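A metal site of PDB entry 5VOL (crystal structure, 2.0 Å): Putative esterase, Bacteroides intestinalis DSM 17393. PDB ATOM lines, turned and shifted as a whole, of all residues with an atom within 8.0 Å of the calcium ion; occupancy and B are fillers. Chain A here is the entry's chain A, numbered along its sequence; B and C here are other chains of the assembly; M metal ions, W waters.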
ATOM      1  N   GLY A 220       8.270 -18.079  18.823  1.00  0.00           N
ATOM      2  CA  GLY A 220       8.128 -18.995  19.966  1.00  0.00           C
ATOM      3  C   GLY A 220       9.091 -20.170  19.997  1.00  0.00           C
ATOM      4  O   GLY A 220       9.575 -20.618  18.933  1.00  0.00           O
ATOM      5  N   ASP A 221       9.380 -20.715  21.185  1.00  0.00           N
ATOM      6  CA  ASP A 221      10.344 -21.812  21.257  1.00  0.00           C
ATOM      7  C   ASP A 221       9.819 -23.112  20.589  1.00  0.00           C
ATOM      8  O   ASP A 221      10.607 -23.969  20.182  1.00  0.00           O
ATOM      9  CB  ASP A 221      10.790 -22.085  22.711  1.00  0.00           C
ATOM     10  CG  ASP A 221       9.675 -22.630  23.612  1.00  0.00           C
ATOM     11  OD1 ASP A 221       8.465 -22.427  23.357  1.00  0.00           O
ATOM     12  OD2 ASP A 221      10.050 -23.253  24.639  1.00  0.00           O
ATOM     13  N   ASP A 222       8.507 -23.229  20.428  1.00  0.00           N
ATOM     14  CA  ASP A 222       7.983 -24.451  19.800  1.00  0.00           C
ATOM     15  C   ASP A 222       7.569 -24.246  18.348  1.00  0.00           C
ATOM     16  O   ASP A 222       6.852 -25.083  17.791  1.00  0.00           O
ATOM     17  CB  ASP A 222       6.788 -24.974  20.609  1.00  0.00           C
ATOM     18  CG  ASP A 222       7.167 -25.269  22.061  1.00  0.00           C
ATOM     19  OD1 ASP A 222       8.219 -25.902  22.285  1.00  0.00           O
ATOM     20  OD2 ASP A 222       6.428 -24.852  22.986  1.00  0.00           O
ATOM     21  N   ASP A 223       8.054 -23.165  17.728  1.00  0.00           N
ATOM     22  CA  ASP A 223       7.664 -22.802  16.361  1.00  0.00           C
ATOM     23  C   ASP A 223       8.541 -23.458  15.295  1.00  0.00           C
ATOM     24  O   ASP A 223       9.766 -23.420  15.408  1.00  0.00           O
ATOM     25  CB  ASP A 223       7.718 -21.287  16.187  1.00  0.00           C
ATOM     26  CG  ASP A 223       6.892 -20.806  15.012  1.00  0.00           C
ATOM     27  OD1 ASP A 223       7.202 -21.182  13.859  1.00  0.00           O
ATOM     28  OD2 ASP A 223       5.906 -20.084  15.236  1.00  0.00           O
ATOM     29  N   VAL A 247      12.484 -14.948  22.138  1.00  0.00           N
ATOM     30  CA  VAL A 247      11.901 -16.278  22.006  1.00  0.00           C
ATOM     31  C   VAL A 247      11.058 -16.507  23.242  1.00  0.00           C
ATOM     32  O   VAL A 247      11.588 -16.679  24.360  1.00  0.00           O
ATOM     33  CB  VAL A 247      12.955 -17.387  21.846  1.00  0.00           C
ATOM     34  CG1 VAL A 247      12.290 -18.769  21.803  1.00  0.00           C
ATOM     35  CG2 VAL A 247      13.794 -17.141  20.579  1.00  0.00           C
ATOM     36  N   ARG A 248       9.748 -16.404  23.071  1.00  0.00           N
ATOM     37  CA  ARG A 248       8.830 -16.595  24.182  1.00  0.00           C
ATOM     38  C   ARG A 248       8.252 -17.999  24.123  1.00  0.00           C
ATOM     39  O   ARG A 248       8.431 -18.698  23.121  1.00  0.00           O
ATOM     40  CB  ARG A 248       7.724 -15.548  24.156  1.00  0.00           C
ATOM     41  CG  ARG A 248       8.261 -14.135  24.165  1.00  0.00           C
ATOM     42  CD  ARG A 248       7.136 -13.135  24.135  1.00  0.00           C
ATOM     43  NE  ARG A 248       6.479 -13.019  22.817  1.00  0.00           N
ATOM     44  CZ  ARG A 248       5.186 -13.242  22.587  1.00  0.00           C
ATOM     45  NH1 ARG A 248       4.380 -13.663  23.573  1.00  0.00           N
ATOM     46  NH2 ARG A 248       4.681 -13.049  21.381  1.00  0.00           N
ATOM     47  N   ASP A 249       7.575 -18.423  25.175  1.00  0.00           N
ATOM     48  CA  ASP A 249       6.940 -19.731  25.165  1.00  0.00           C
ATOM     49  C   ASP A 249       5.892 -19.771  24.062  1.00  0.00           C
ATOM     50  O   ASP A 249       5.105 -18.848  23.932  1.00  0.00           O
ATOM     51  CB  ASP A 249       6.289 -20.030  26.518  1.00  0.00           C
ATOM     52  CG  ASP A 249       5.716 -21.449  26.582  1.00  0.00           C
ATOM     53  OD1 ASP A 249       6.328 -22.346  25.982  1.00  0.00           O
ATOM     54  OD2 ASP A 249       4.680 -21.654  27.234  1.00  0.00           O
ATOM     55  N   GLY A 250       5.855 -20.849  23.290  1.00  0.00           N
ATOM     56  CA  GLY A 250       4.765 -21.003  22.353  1.00  0.00           C
ATOM     57  C   GLY A 250       5.115 -21.412  20.948  1.00  0.00           C
ATOM     58  O   GLY A 250       6.277 -21.622  20.590  1.00  0.00           O
ATOM     59  N   GLY A 251       4.077 -21.546  20.136  1.00  0.00           N
ATOM     60  CA  GLY A 251       4.216 -22.088  18.807  1.00  0.00           C
ATOM     61  C   GLY A 251       3.625 -21.171  17.765  1.00  0.00           C
ATOM     62  O   GLY A 251       3.470 -19.963  17.979  1.00  0.00           O
ATOM     63  N   PHE B 216      14.969 -26.285  31.436  1.00  0.00           N
ATOM     64  CA  PHE B 216      14.592 -24.914  31.155  1.00  0.00           C
ATOM     65  C   PHE B 216      15.873 -24.141  30.821  1.00  0.00           C
ATOM     66  O   PHE B 216      16.780 -24.114  31.635  1.00  0.00           O
ATOM     67  CB  PHE B 216      13.875 -24.303  32.359  1.00  0.00           C
ATOM     68  CG  PHE B 216      13.000 -23.122  32.028  1.00  0.00           C
ATOM     69  CD1 PHE B 216      13.533 -21.954  31.510  1.00  0.00           C
ATOM     70  CD2 PHE B 216      11.635 -23.180  32.273  1.00  0.00           C
ATOM     71  CE1 PHE B 216      12.728 -20.872  31.232  1.00  0.00           C
ATOM     72  CE2 PHE B 216      10.808 -22.089  31.986  1.00  0.00           C
ATOM     73  CZ  PHE B 216      11.357 -20.938  31.460  1.00  0.00           C
ATOM     74  N   TYR B 233      19.604 -26.121  22.652  1.00  0.00           N
ATOM     75  CA  TYR B 233      18.161 -26.263  22.521  1.00  0.00           C
ATOM     76  C   TYR B 233      17.806 -27.029  21.229  1.00  0.00           C
ATOM     77  O   TYR B 233      16.968 -27.935  21.237  1.00  0.00           O
ATOM     78  CB  TYR B 233      17.465 -24.905  22.533  1.00  0.00           C
ATOM     79  CG  TYR B 233      15.977 -25.060  22.352  1.00  0.00           C
ATOM     80  CD1 TYR B 233      15.228 -25.805  23.266  1.00  0.00           C
ATOM     81  CD2 TYR B 233      15.324 -24.520  21.257  1.00  0.00           C
ATOM     82  CE1 TYR B 233      13.868 -25.974  23.111  1.00  0.00           C
ATOM     83  CE2 TYR B 233      13.948 -24.706  21.092  1.00  0.00           C
ATOM     84  CZ  TYR B 233      13.227 -25.422  22.018  1.00  0.00           C
ATOM     85  OH  TYR B 233      11.867 -25.591  21.863  1.00  0.00           O
ATOM     86  N   CYS B 243      12.028 -29.506  26.357  1.00  0.00           N
ATOM     87  CA  CYS B 243      12.872 -28.475  26.925  1.00  0.00           C
ATOM     88  C   CYS B 243      12.223 -27.107  26.683  1.00  0.00           C
ATOM     89  O   CYS B 243      11.792 -26.845  25.570  1.00  0.00           O
ATOM     90  CB  CYS B 243      14.266 -28.531  26.297  1.00  0.00           C
ATOM     91  SG  CYS B 243      15.504 -27.357  26.949  1.00  0.00           S
ATOM     92  N   GLN B 244      12.135 -26.271  27.714  1.00  0.00           N
ATOM     93  CA  GLN B 244      11.684 -24.890  27.510  1.00  0.00           C
ATOM     94  C   GLN B 244      12.877 -24.015  27.126  1.00  0.00           C
ATOM     95  O   GLN B 244      13.964 -24.171  27.676  1.00  0.00           O
ATOM     96  CB  GLN B 244      10.992 -24.331  28.768  1.00  0.00           C
ATOM     97  CG  GLN B 244       9.764 -25.126  29.214  1.00  0.00           C
ATOM     98  CD  GLN B 244       8.678 -25.140  28.155  1.00  0.00           C
ATOM     99  OE1 GLN B 244       8.461 -24.138  27.467  1.00  0.00           O
ATOM    100  NE2 GLN B 244       8.015 -26.277  27.996  1.00  0.00           N
ATOM    101  N   PHE B 245      12.667 -23.083  26.203  1.00  0.00           N
ATOM    102  CA  PHE B 245      13.730 -22.163  25.767  1.00  0.00           C
ATOM    103  C   PHE B 245      13.156 -20.756  25.774  1.00  0.00           C
ATOM    104  O   PHE B 245      12.064 -20.531  25.248  1.00  0.00           O
ATOM    105  CB  PHE B 245      14.239 -22.556  24.362  1.00  0.00           C
ATOM    106  CG  PHE B 245      15.417 -21.733  23.858  1.00  0.00           C
ATOM    107  CD1 PHE B 245      16.473 -21.393  24.697  1.00  0.00           C
ATOM    108  CD2 PHE B 245      15.474 -21.345  22.527  1.00  0.00           C
ATOM    109  CE1 PHE B 245      17.570 -20.639  24.208  1.00  0.00           C
ATOM    110  CE2 PHE B 245      16.559 -20.594  22.031  1.00  0.00           C
ATOM    111  CZ  PHE B 245      17.608 -20.248  22.881  1.00  0.00           C
ATOM    112  N   ARG B 246      13.853 -19.838  26.459  1.00  0.00           N
ATOM    113  CA  ARG B 246      13.456 -18.424  26.512  1.00  0.00           C
ATOM    114  C   ARG B 246      14.652 -17.577  26.119  1.00  0.00           C
ATOM    115  O   ARG B 246      15.757 -17.763  26.632  1.00  0.00           O
ATOM    116  CB  ARG B 246      12.960 -18.002  27.909  1.00  0.00           C
ATOM    117  CG  ARG B 246      11.794 -18.796  28.488  1.00  0.00           C
ATOM    118  CD  ARG B 246      10.477 -18.693  27.698  1.00  0.00           C
ATOM    119  NE  ARG B 246       9.480 -19.518  28.357  1.00  0.00           N
ATOM    120  CZ  ARG B 246       9.185 -20.781  28.031  1.00  0.00           C
ATOM    121  NH1 ARG B 246       9.778 -21.358  26.988  1.00  0.00           N
ATOM    122  NH2 ARG B 246       8.284 -21.461  28.736  1.00  0.00           N
ATOM    123  N   ARG C  72      -1.546 -23.801  25.650  1.00  0.00           N
ATOM    124  CA  ARG C  72      -0.266 -23.191  26.009  1.00  0.00           C
ATOM    125  C   ARG C  72       0.199 -23.638  27.395  1.00  0.00           C
ATOM    126  O   ARG C  72       1.305 -24.159  27.556  1.00  0.00           O
ATOM    127  CB  ARG C  72      -0.368 -21.662  25.958  1.00  0.00           C
ATOM    128  CG  ARG C  72       0.886 -20.922  26.433  1.00  0.00           C
ATOM    129  CD  ARG C  72       1.994 -20.889  25.357  1.00  0.00           C
ATOM    130  NE  ARG C  72       1.771 -19.854  24.348  1.00  0.00           N
ATOM    131  CZ  ARG C  72       1.455 -20.077  23.078  1.00  0.00           C
ATOM    132  NH1 ARG C  72       1.297 -21.324  22.619  1.00  0.00           N
ATOM    133  NH2 ARG C  72       1.278 -19.023  22.256  1.00  0.00           N
ATOM    134  N   ALA C  75       1.079 -27.348  28.002  1.00  0.00           N
ATOM    135  CA  ALA C  75       2.336 -27.715  27.356  1.00  0.00           C
ATOM    136  C   ALA C  75       3.556 -27.274  28.162  1.00  0.00           C
ATOM    137  O   ALA C  75       4.578 -27.952  28.150  1.00  0.00           O
ATOM    138  CB  ALA C  75       2.411 -27.123  25.960  1.00  0.00           C
ATOM    139  N   SER C  76       3.468 -26.143  28.852  1.00  0.00           N
ATOM    140  CA  SER C  76       4.606 -25.624  29.607  1.00  0.00           C
ATOM    141  C   SER C  76       4.628 -26.152  31.022  1.00  0.00           C
ATOM    142  O   SER C  76       5.585 -25.914  31.770  1.00  0.00           O
ATOM    143  CB  SER C  76       4.584 -24.099  29.638  1.00  0.00           C
ATOM    144  OG  SER C  76       3.458 -23.622  30.372  1.00  0.00           O
ATOM    145  N   GLU C  78       2.574 -25.105  33.339  1.00  0.00           N
ATOM    146  CA  GLU C  78       2.075 -24.094  34.267  1.00  0.00           C
ATOM    147  C   GLU C  78       0.631 -24.341  34.705  1.00  0.00           C
ATOM    148  O   GLU C  78       0.232 -23.891  35.777  1.00  0.00           O
ATOM    149  CB  GLU C  78       2.190 -22.695  33.666  1.00  0.00           C
ATOM    150  CG  GLU C  78       3.603 -22.177  33.587  1.00  0.00           C
ATOM    151  CD  GLU C  78       3.697 -20.953  32.698  1.00  0.00           C
ATOM    152  OE1 GLU C  78       3.354 -19.848  33.153  1.00  0.00           O
ATOM    153  OE2 GLU C  78       4.098 -21.108  31.519  1.00  0.00           O
HETATM  154 CA    CA M   1       7.686 -24.067  25.121  1.00  0.00          CA
HETATM  155  O   HOH W   1       9.069 -26.173  24.688  1.00  0.00           O
HETATM  156  O   HOH W   2       5.771 -25.574  25.778  1.00  0.00           O
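Arg 246 of chain B touches the calcium ion.
The nearest printed residue that does not touch the calcium ion is Gly 250 (4.1 Å).
The backbone carbonyl oxygen (O) of Gly 250 sits at hydrogen-bond distance from the backbone NH (N) of Asp 222, at 2.8 Å.
The side-chain amide oxygen (OE1) of Gln 244 of chain B lies close to the guanidinium group (NH2) of Arg 246 of chain B.
OH of Tyr 233 of chain B sits at hydrogen-bond distance from O of Asp 221.
The backbone NH of Asp 221 lies within hydrogen-bond range of the backbone carbonyl oxygen of Gly 250 (3.3 Å).
OD2 of Asp 221 lies close to NH1 of Arg 246 of chain B (3.0 Å).
The guanidinium group (NH2) of Arg 246 of chain B lies within salt-bridge range of the side-chain carboxylate (OD2) of Asp 249.
N of Asp 221 lies within hydrogen-bond range of O of Arg 248, 3.0 Å away.
The side-chain carboxylate (OD2) of Asp 221 lies close to the backbone NH (N) of Phe 245 of chain B, at 3.1 Å.
The calcium ion is bound by the side-chain carboxylate (OD1) of Asp 249, the side-chain amide oxygen (OE1) of Gln 244 of chain B, water W2, the side-chain carboxylate (OD1) of Asp 221, the side-chain carboxylate (OD2) of Asp 221, water W1 and the side-chain carboxylate (OD2) of Asp 222.
The calcium ion has seven donor atoms within binding distance.
Water W1 lies within hydrogen-bond range of the side-chain carboxylate (OD1) of Asp 222 (2.6 Å), the backbone carbonyl oxygen (O) of Cys 243 of chain B (2.9 Å) and the side-chain amide nitrogen (NE2) of Gln 244 of chain B (3.5 Å).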
